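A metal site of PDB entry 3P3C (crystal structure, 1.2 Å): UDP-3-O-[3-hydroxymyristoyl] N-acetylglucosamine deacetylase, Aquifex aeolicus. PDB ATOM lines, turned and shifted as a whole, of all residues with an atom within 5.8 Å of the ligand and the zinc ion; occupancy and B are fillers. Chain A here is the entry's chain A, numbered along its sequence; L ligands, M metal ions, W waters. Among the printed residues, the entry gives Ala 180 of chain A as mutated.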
ATOM      1  N   ILE A  17     -11.742  30.756 -11.179  1.00  0.00           N
ATOM      2  CA  ILE A  17     -10.478  30.152 -10.816  1.00  0.00           C
ATOM      3  C   ILE A  17      -9.642  31.001  -9.846  1.00  0.00           C
ATOM      4  O   ILE A  17      -8.926  30.460  -9.018  1.00  0.00           O
ATOM      5  CB  ILE A  17      -9.643  29.782 -12.059  1.00  0.00           C
ATOM      6  CG1 ILE A  17      -8.602  28.725 -11.689  1.00  0.00           C
ATOM      7  CG2 ILE A  17      -8.996  31.017 -12.670  1.00  0.00           C
ATOM      8  CD1 ILE A  17      -7.809  28.206 -12.857  1.00  0.00           C
ATOM      9  N   HIS A  18      -9.742  32.323  -9.948  1.00  0.00           N
ATOM     10  CA  HIS A  18      -8.945  33.184  -9.083  1.00  0.00           C
ATOM     11  C   HIS A  18      -9.652  33.665  -7.821  1.00  0.00           C
ATOM     12  O   HIS A  18      -9.052  33.677  -6.756  1.00  0.00           O
ATOM     13  CB  HIS A  18      -8.383  34.366  -9.872  1.00  0.00           C
ATOM     14  CG  HIS A  18      -7.363  33.966 -10.871  1.00  0.00           C
ATOM     15  ND1 HIS A  18      -6.235  33.253 -10.521  1.00  0.00           N
ATOM     16  CD2 HIS A  18      -7.300  34.123 -12.216  1.00  0.00           C
ATOM     17  CE1 HIS A  18      -5.514  33.013 -11.603  1.00  0.00           C
ATOM     18  NE2 HIS A  18      -6.147  33.522 -12.640  1.00  0.00           N
ATOM     19  N   HIS A  57      -1.665  36.683 -14.483  1.00  0.00           N
ATOM     20  CA  HIS A  57      -2.318  35.374 -14.359  1.00  0.00           C
ATOM     21  C   HIS A  57      -3.719  35.317 -14.957  1.00  0.00           C
ATOM     22  O   HIS A  57      -4.323  34.242 -15.053  1.00  0.00           O
ATOM     23  CB  HIS A  57      -2.336  34.881 -12.913  1.00  0.00           C
ATOM     24  CG  HIS A  57      -0.986  34.773 -12.300  1.00  0.00           C
ATOM     25  ND1 HIS A  57      -0.128  33.722 -12.568  1.00  0.00           N
ATOM     26  CD2 HIS A  57      -0.324  35.585 -11.442  1.00  0.00           C
ATOM     27  CE1 HIS A  57       0.992  33.895 -11.890  1.00  0.00           C
ATOM     28  NE2 HIS A  57       0.899  35.023 -11.196  1.00  0.00           N
ATOM     29  N   SER A  58      -4.257  36.467 -15.342  1.00  0.00           N
ATOM     30  CA  SER A  58      -5.518  36.555 -16.066  1.00  0.00           C
ATOM     31  C   SER A  58      -5.626  37.934 -16.651  1.00  0.00           C
ATOM     32  O   SER A  58      -4.873  38.833 -16.294  1.00  0.00           O
ATOM     33  CB  SER A  58      -6.718  36.287 -15.135  1.00  0.00           C
ATOM     34  OG  SER A  58      -6.841  37.299 -14.149  1.00  0.00           O
ATOM     35  N   THR A  70     -10.790  37.542 -15.471  1.00  0.00           N
ATOM     36  CA  THR A  70     -10.578  36.341 -16.266  1.00  0.00           C
ATOM     37  C   THR A  70     -11.507  36.273 -17.475  1.00  0.00           C
ATOM     38  O   THR A  70     -12.295  35.340 -17.621  1.00  0.00           O
ATOM     39  CB  THR A  70     -10.712  35.075 -15.408  1.00  0.00           C
ATOM     40  OG1 THR A  70     -10.025  35.292 -14.164  1.00  0.00           O
ATOM     41  CG2 THR A  70     -10.114  33.869 -16.107  1.00  0.00           C
ATOM     42  N   GLU A  72     -10.454  36.115 -20.607  1.00  0.00           N
ATOM     43  CA  GLU A  72      -9.737  35.643 -21.784  1.00  0.00           C
ATOM     44  C   GLU A  72     -10.337  34.401 -22.455  1.00  0.00           C
ATOM     45  O   GLU A  72     -10.275  34.269 -23.669  1.00  0.00           O
ATOM     46  CB  GLU A  72      -8.251  35.407 -21.468  1.00  0.00           C
ATOM     47  CG  GLU A  72      -7.972  34.381 -20.375  1.00  0.00           C
ATOM     48  CD  GLU A  72      -7.800  35.005 -18.997  1.00  0.00           C
ATOM     49  OE1 GLU A  72      -8.330  36.104 -18.742  1.00  0.00           O
ATOM     50  OE2 GLU A  72      -7.125  34.369 -18.153  1.00  0.00           O
ATOM     51  N   HIS A  73     -10.918  33.492 -21.674  1.00  0.00           N
ATOM     52  CA  HIS A  73     -11.412  32.242 -22.241  1.00  0.00           C
ATOM     53  C   HIS A  73     -12.750  32.418 -22.965  1.00  0.00           C
ATOM     54  O   HIS A  73     -12.936  31.897 -24.062  1.00  0.00           O
ATOM     55  CB  HIS A  73     -11.497  31.168 -21.163  1.00  0.00           C
ATOM     56  CG  HIS A  73     -10.216  31.002 -20.399  1.00  0.00           C
ATOM     57  ND1 HIS A  73     -10.181  30.880 -19.026  1.00  0.00           N
ATOM     58  CD2 HIS A  73      -8.930  30.956 -20.813  1.00  0.00           C
ATOM     59  CE1 HIS A  73      -8.927  30.757 -18.622  1.00  0.00           C
ATOM     60  NE2 HIS A  73      -8.148  30.796 -19.695  1.00  0.00           N
ATOM     61  N   GLY A 100     -11.761  24.375 -17.163  1.00  0.00           N
ATOM     62  CA  GLY A 100     -10.441  24.930 -17.420  1.00  0.00           C
ATOM     63  C   GLY A 100     -10.203  25.279 -18.879  1.00  0.00           C
ATOM     64  O   GLY A 100      -9.216  25.929 -19.198  1.00  0.00           O
ATOM     65  N   THR A 178      -6.332  25.466 -18.837  1.00  0.00           N
ATOM     66  CA  THR A 178      -5.370  26.257 -18.096  1.00  0.00           C
ATOM     67  C   THR A 178      -4.512  25.321 -17.247  1.00  0.00           C
ATOM     68  O   THR A 178      -4.940  24.219 -16.891  1.00  0.00           O
ATOM     69  CB  THR A 178      -6.093  27.283 -17.210  1.00  0.00           C
ATOM     70  OG1 THR A 178      -5.149  28.214 -16.682  1.00  0.00           O
ATOM     71  CG2 THR A 178      -6.829  26.602 -16.061  1.00  0.00           C
ATOM     72  N   PHE A 179      -3.299  25.758 -16.937  1.00  0.00           N
ATOM     73  CA  PHE A 179      -2.333  24.914 -16.261  1.00  0.00           C
ATOM     74  C   PHE A 179      -1.506  25.715 -15.273  1.00  0.00           C
ATOM     75  O   PHE A 179      -1.427  26.940 -15.370  1.00  0.00           O
ATOM     76  CB  PHE A 179      -1.422  24.219 -17.276  1.00  0.00           C
ATOM     77  CG  PHE A 179      -0.590  25.159 -18.107  1.00  0.00           C
ATOM     78  CD1 PHE A 179       0.708  25.462 -17.742  1.00  0.00           C
ATOM     79  CD2 PHE A 179      -1.121  25.750 -19.235  1.00  0.00           C
ATOM     80  CE1 PHE A 179       1.475  26.336 -18.503  1.00  0.00           C
ATOM     81  CE2 PHE A 179      -0.368  26.624 -20.001  1.00  0.00           C
ATOM     82  CZ  PHE A 179       0.930  26.917 -19.634  1.00  0.00           C
ATOM     83  N   ALA A 180      -0.909  25.018 -14.318  1.00  0.00           N
ATOM     84  CA  ALA A 180      -0.050  25.625 -13.322  1.00  0.00           C
ATOM     85  C   ALA A 180       1.002  24.636 -12.883  1.00  0.00           C
ATOM     86  O   ALA A 180       0.807  23.421 -12.975  1.00  0.00           O
ATOM     87  CB  ALA A 180      -0.871  26.090 -12.125  1.00  0.00           C
ATOM     88  N   ILE A 185       2.395  27.554  -7.239  1.00  0.00           N
ATOM     89  CA  ILE A 185       1.041  27.738  -6.731  1.00  0.00           C
ATOM     90  C   ILE A 185       1.000  28.479  -5.387  1.00  0.00           C
ATOM     91  O   ILE A 185       0.100  29.278  -5.149  1.00  0.00           O
ATOM     92  CB  ILE A 185       0.286  26.394  -6.642  1.00  0.00           C
ATOM     93  CG1 ILE A 185      -0.041  25.893  -8.051  1.00  0.00           C
ATOM     94  CG2 ILE A 185      -1.003  26.555  -5.840  1.00  0.00           C
ATOM     95  CD1 ILE A 185      -0.651  24.511  -8.090  1.00  0.00           C
ATOM     96  N   ILE A 188       1.191  32.172  -6.093  1.00  0.00           N
ATOM     97  CA  ILE A 188      -0.036  32.631  -6.723  1.00  0.00           C
ATOM     98  C   ILE A 188      -1.128  32.841  -5.676  1.00  0.00           C
ATOM     99  O   ILE A 188      -1.839  33.835  -5.704  1.00  0.00           O
ATOM    100  CB  ILE A 188      -0.489  31.652  -7.812  1.00  0.00           C
ATOM    101  CG1 ILE A 188       0.517  31.680  -8.966  1.00  0.00           C
ATOM    102  CG2 ILE A 188      -1.879  32.010  -8.308  1.00  0.00           C
ATOM    103  CD1 ILE A 188       0.295  30.623 -10.021  1.00  0.00           C
ATOM    104  N   LYS A 189      -1.240  31.906  -4.738  1.00  0.00           N
ATOM    105  CA  LYS A 189      -2.227  32.046  -3.683  1.00  0.00           C
ATOM    106  C   LYS A 189      -1.866  33.190  -2.738  1.00  0.00           C
ATOM    107  O   LYS A 189      -2.738  33.912  -2.263  1.00  0.00           O
ATOM    108  CB  LYS A 189      -2.379  30.732  -2.915  1.00  0.00           C
ATOM    109  CG  LYS A 189      -3.028  29.628  -3.749  1.00  0.00           C
ATOM    110  CD  LYS A 189      -3.389  28.434  -2.893  1.00  0.00           C
ATOM    111  CE  LYS A 189      -4.244  27.446  -3.676  1.00  0.00           C
ATOM    112  NZ  LYS A 189      -4.843  26.399  -2.798  1.00  0.00           N
ATOM    113  N   GLY A 194      -5.776  32.378  -7.665  1.00  0.00           N
ATOM    114  CA  GLY A 194      -5.894  30.931  -7.691  1.00  0.00           C
ATOM    115  C   GLY A 194      -6.796  30.295  -6.641  1.00  0.00           C
ATOM    116  O   GLY A 194      -6.684  29.099  -6.396  1.00  0.00           O
ATOM    117  N   GLY A 197      -8.769  27.320  -7.962  1.00  0.00           N
ATOM    118  CA  GLY A 197      -8.026  26.318  -8.703  1.00  0.00           C
ATOM    119  C   GLY A 197      -8.057  24.950  -8.037  1.00  0.00           C
ATOM    120  O   GLY A 197      -7.900  24.839  -6.829  1.00  0.00           O
ATOM    121  N   SER A 198      -8.264  23.919  -8.843  1.00  0.00           N
ATOM    122  CA  SER A 198      -8.269  22.540  -8.347  1.00  0.00           C
ATOM    123  C   SER A 198      -7.963  21.613  -9.511  1.00  0.00           C
ATOM    124  O   SER A 198      -7.879  22.043 -10.648  1.00  0.00           O
ATOM    125  CB  SER A 198      -9.643  22.177  -7.782  1.00  0.00           C
ATOM    126  OG  SER A 198     -10.562  21.934  -8.828  1.00  0.00           O
ATOM    127  N   LEU A 199      -7.796  20.336  -9.221  1.00  0.00           N
ATOM    128  CA  LEU A 199      -7.553  19.356 -10.271  1.00  0.00           C
ATOM    129  C   LEU A 199      -8.781  19.170 -11.162  1.00  0.00           C
ATOM    130  O   LEU A 199      -8.696  18.520 -12.197  1.00  0.00           O
ATOM    131  CB  LEU A 199      -7.118  18.018  -9.675  1.00  0.00           C
ATOM    132  CG  LEU A 199      -5.810  18.044  -8.892  1.00  0.00           C
ATOM    133  CD1 LEU A 199      -5.426  16.645  -8.424  1.00  0.00           C
ATOM    134  CD2 LEU A 199      -4.682  18.652  -9.730  1.00  0.00           C
ATOM    135  N   THR A 202      -7.881  22.682 -13.510  1.00  0.00           N
ATOM    136  CA  THR A 202      -6.522  23.075 -13.821  1.00  0.00           C
ATOM    137  C   THR A 202      -5.652  21.857 -14.039  1.00  0.00           C
ATOM    138  O   THR A 202      -5.713  20.899 -13.261  1.00  0.00           O
ATOM    139  CB  THR A 202      -5.902  23.875 -12.660  1.00  0.00           C
ATOM    140  OG1 THR A 202      -6.721  25.016 -12.362  1.00  0.00           O
ATOM    141  CG2 THR A 202      -4.504  24.361 -13.009  1.00  0.00           C
ATOM    142  N   VAL A 204      -2.367  20.509 -13.398  1.00  0.00           N
ATOM    143  CA  VAL A 204      -1.296  20.837 -12.458  1.00  0.00           C
ATOM    144  C   VAL A 204      -0.106  19.911 -12.689  1.00  0.00           C
ATOM    145  O   VAL A 204      -0.230  18.693 -12.660  1.00  0.00           O
ATOM    146  CB  VAL A 204      -1.780  20.732 -11.003  1.00  0.00           C
ATOM    147  CG1 VAL A 204      -0.647  21.056 -10.049  1.00  0.00           C
ATOM    148  CG2 VAL A 204      -2.955  21.678 -10.770  1.00  0.00           C
ATOM    149  N   HIS A 225      -3.206  25.754 -24.907  1.00  0.00           N
ATOM    150  CA  HIS A 225      -3.932  26.694 -24.070  1.00  0.00           C
ATOM    151  C   HIS A 225      -3.364  28.103 -24.191  1.00  0.00           C
ATOM    152  O   HIS A 225      -4.122  29.076 -24.171  1.00  0.00           O
ATOM    153  CB  HIS A 225      -3.939  26.273 -22.601  1.00  0.00           C
ATOM    154  CG  HIS A 225      -4.817  27.136 -21.772  1.00  0.00           C
ATOM    155  ND1 HIS A 225      -6.184  26.977 -21.729  1.00  0.00           N
ATOM    156  CD2 HIS A 225      -4.545  28.237 -21.014  1.00  0.00           C
ATOM    157  CE1 HIS A 225      -6.713  27.913 -20.947  1.00  0.00           C
ATOM    158  NE2 HIS A 225      -5.739  28.688 -20.515  1.00  0.00           N
ATOM    159  N   LYS A 226      -2.044  28.239 -24.298  1.00  0.00           N
ATOM    160  CA  LYS A 226      -1.445  29.552 -24.440  1.00  0.00           C
ATOM    161  C   LYS A 226      -1.883  30.215 -25.743  1.00  0.00           C
ATOM    162  O   LYS A 226      -2.083  31.431 -25.787  1.00  0.00           O
ATOM    163  CB  LYS A 226       0.077  29.447 -24.365  1.00  0.00           C
ATOM    164  CG  LYS A 226       0.610  29.324 -22.942  1.00  0.00           C
ATOM    165  CD  LYS A 226       0.560  30.673 -22.228  1.00  0.00           C
ATOM    166  CE  LYS A 226       1.213  30.623 -20.860  1.00  0.00           C
ATOM    167  NZ  LYS A 226       1.225  31.967 -20.222  1.00  0.00           N
ATOM    168  N   PHE A 228      -4.805  29.621 -27.174  1.00  0.00           N
ATOM    169  CA  PHE A 228      -6.185  29.961 -26.832  1.00  0.00           C
ATOM    170  C   PHE A 228      -6.247  31.279 -26.042  1.00  0.00           C
ATOM    171  O   PHE A 228      -7.063  32.149 -26.357  1.00  0.00           O
ATOM    172  CB  PHE A 228      -6.791  28.780 -26.065  1.00  0.00           C
ATOM    173  CG  PHE A 228      -8.215  28.985 -25.613  1.00  0.00           C
ATOM    174  CD1 PHE A 228      -9.269  28.933 -26.512  1.00  0.00           C
ATOM    175  CD2 PHE A 228      -8.503  29.153 -24.274  1.00  0.00           C
ATOM    176  CE1 PHE A 228     -10.576  29.084 -26.081  1.00  0.00           C
ATOM    177  CE2 PHE A 228      -9.797  29.303 -23.840  1.00  0.00           C
ATOM    178  CZ  PHE A 228     -10.840  29.269 -24.745  1.00  0.00           C
ATOM    179  N   ASP A 229      -5.390  31.441 -25.050  1.00  0.00           N
ATOM    180  CA  ASP A 229      -5.305  32.691 -24.286  1.00  0.00           C
ATOM    181  C   ASP A 229      -5.021  33.888 -25.182  1.00  0.00           C
ATOM    182  O   ASP A 229      -5.655  34.930 -25.073  1.00  0.00           O
ATOM    183  CB  ASP A 229      -4.169  32.619 -23.252  1.00  0.00           C
ATOM    184  CG  ASP A 229      -4.558  31.899 -21.985  1.00  0.00           C
ATOM    185  OD1 ASP A 229      -5.759  31.655 -21.741  1.00  0.00           O
ATOM    186  OD2 ASP A 229      -3.629  31.576 -21.201  1.00  0.00           O
ATOM    187  N   HIS A 252      -0.316  37.266 -20.679  1.00  0.00           N
ATOM    188  CA  HIS A 252      -1.334  38.292 -20.857  1.00  0.00           C
ATOM    189  C   HIS A 252      -0.748  39.695 -20.919  1.00  0.00           C
ATOM    190  O   HIS A 252      -1.208  40.519 -21.705  1.00  0.00           O
ATOM    191  CB  HIS A 252      -2.375  38.232 -19.739  1.00  0.00           C
ATOM    192  CG  HIS A 252      -3.068  36.923 -19.651  1.00  0.00           C
ATOM    193  ND1 HIS A 252      -3.846  36.416 -20.672  1.00  0.00           N
ATOM    194  CD2 HIS A 252      -3.099  35.995 -18.665  1.00  0.00           C
ATOM    195  CE1 HIS A 252      -4.325  35.239 -20.307  1.00  0.00           C
ATOM    196  NE2 HIS A 252      -3.878  34.958 -19.101  1.00  0.00           N
HETATM  197  O1  LIG L   1      -4.850  30.365 -18.243  1.00  0.00           O
HETATM  198  C1  LIG L   1      -4.169  31.307 -17.841  1.00  0.00           C
HETATM  199  N1  LIG L   1      -4.630  32.566 -18.171  1.00  0.00           N
HETATM  200  O2  LIG L   1      -5.697  32.517 -18.962  1.00  0.00           O
HETATM  201  C2  LIG L   1      -2.968  31.204 -16.939  1.00  0.00           C
HETATM  202  N2  LIG L   1      -3.342  30.502 -15.760  1.00  0.00           N
HETATM  203  C3  LIG L   1      -2.856  30.875 -14.469  1.00  0.00           C
HETATM  204  O3  LIG L   1      -2.013  31.675 -14.376  1.00  0.00           O
HETATM  205  C4  LIG L   1      -3.253  30.023 -13.291  1.00  0.00           C
HETATM  206  C5  LIG L   1      -4.142  28.975 -13.468  1.00  0.00           C
HETATM  207  C6  LIG L   1      -4.445  28.111 -12.415  1.00  0.00           C
HETATM  208  C7  LIG L   1      -3.873  28.299 -11.167  1.00  0.00           C
HETATM  209  C8  LIG L   1      -2.980  29.347 -10.981  1.00  0.00           C
HETATM  210  C9  LIG L   1      -2.676  30.221 -12.035  1.00  0.00           C
HETATM  211  C10 LIG L   1      -4.063  27.258 -10.150  1.00  0.00           C
HETATM  212  C11 LIG L   1      -4.207  26.415  -9.326  1.00  0.00           C
HETATM  213  C12 LIG L   1      -4.331  25.404  -8.433  1.00  0.00           C
HETATM  214  C13 LIG L   1      -4.426  24.498  -7.675  1.00  0.00           C
HETATM  215  C14 LIG L   1      -4.526  23.408  -6.756  1.00  0.00           C
HETATM  216  C15 LIG L   1      -4.859  22.144  -7.224  1.00  0.00           C
HETATM  217  C16 LIG L   1      -4.965  21.082  -6.326  1.00  0.00           C
HETATM  218  C17 LIG L   1      -4.742  21.294  -4.970  1.00  0.00           C
HETATM  219  C18 LIG L   1      -4.412  22.568  -4.512  1.00  0.00           C
HETATM  220  C19 LIG L   1      -4.307  23.619  -5.409  1.00  0.00           C
HETATM  221  C20 LIG L   1      -1.786  30.622 -17.717  1.00  0.00           C
HETATM  222  C21 LIG L   1      -2.083  29.120 -17.929  1.00  0.00           C
HETATM  223  O4  LIG L   1      -1.649  31.337 -18.968  1.00  0.00           O
HETATM  224 ZN    ZN M   1      -6.033  30.685 -19.898  1.00  0.00          ZN
HETATM  225  O   HOH W   1       1.024  31.317 -13.853  1.00  0.00           O
HETATM  226  O   HOH W   2      -0.400  33.451 -16.469  1.00  0.00           O
HETATM  227  O   HOH W   3      -1.391  33.500 -21.542  1.00  0.00           O
HETATM  228  O   HOH W   4      -7.177  30.264 -15.963  1.00  0.00           O
HETATM  229  O   HOH W   5      -6.558  32.951 -15.732  1.00  0.00           O
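CD1 of Ile 17 touches C6 of the ligand, 3.4 Å away. O of Phe 179 touches C21 of the ligand (3.4 Å). Ala 180 touches the ligand. Ile 185 touches the ligand. CD1 of Ile 188 touches C9 of the ligand, 3.6 Å away. Lys 189 touches the ligand. Gly 197 touches the ligand (O to C13, 3.6 Å). Ser 198 touches the ligand (CA to C15, 3.6 Å). N of Leu 199 touches C15 of the ligand (3.99 Å). CG2 of Thr 202 touches C6 of the ligand, 3.8 Å away. Hydrophobic or aromatic side chains that line the ligand: Ile 17, His 57, His 73, Phe 179, Ala 180, Ile 185, Ile 188, His 225 and His 252. Within 4 Å of the ligand: Ile 17, His 57, Glu 72, His 73, Thr 178, Phe 179, Ala 180, Ile 185, Ile 188, Lys 189, Gly 197, Ser 198, Leu 199, Thr 202, His 225, Lys 226, Asp 229 and His 252. The nearest printed residue that does not touch the ligand is His 18 (4.005 Å).
Water W1 lies within hydrogen-bond range of a ring nitrogen (ND1) of His 57 (3.0 Å) and an oxygen (O3) of the ligand (3.1 Å). Water W5 lies within hydrogen-bond range of the backbone carbonyl oxygen of His 57 (2.7 Å), the side-chain carboxylate of Glu 72 (2.9 Å), a nitrogen (N1) of the ligand (3.1 Å) and a ring nitrogen (NE2) of His 18 (3.2 Å). Water W3 lies within hydrogen-bond range of the side-chain carboxylate of Asp 229, the side-chain amino group of Lys 226 and an oxygen (O4) of the ligand.
OE2 of Glu 72 lies within hydrogen-bond range of N1 of the ligand (3.1 Å). NE2 of His 252 lies within hydrogen-bond range of N1 of the ligand. A nitrogen (N2) of the ligand is in hydrogen-bond range of the side-chain hydroxyl (OG1) of Thr 178, at 3.1 Å. The side-chain amino group (NZ) of Lys 226 sits at hydrogen-bond distance from an oxygen (O4) of the ligand, at 3.2 Å. An oxygen (O3) of the ligand lies within hydrogen-bond range of a ring nitrogen (ND1) of His 57, at 3.3 Å.
ND1 of His 225 sits close to N of Thr 178, 3.3 Å away. The side-chain carboxylate (OE2) of Glu 72 lies within hydrogen-bond range of a ring nitrogen (NE2) of His 252, 3.4 Å away. O of Gly 100 is in hydrogen-bond range of N of Thr 178 (2.9 Å). A ring nitrogen (NE2) of His 18 is in hydrogen-bond range of the backbone carbonyl oxygen (O) of His 57 (3.1 Å). O of Ile 17 lies within hydrogen-bond range of N of Gly 197, at 3.3 Å.
The zinc ion is bound by O1 of the ligand (2.1 Å), O2 of the ligand (2.1 Å), OD1 of Asp 229 (2.1 Å), NE2 of His 225 (2.1 Å) and NE2 of His 73 (2.1 Å). The zinc ion has five donor atoms within binding distance.
Three residues have an atom within 4 Å of the zinc ion: His 73, His 225 and Asp 229. The nearest printed residue that does not touch the zinc ion is Thr 178 (4.2 Å).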
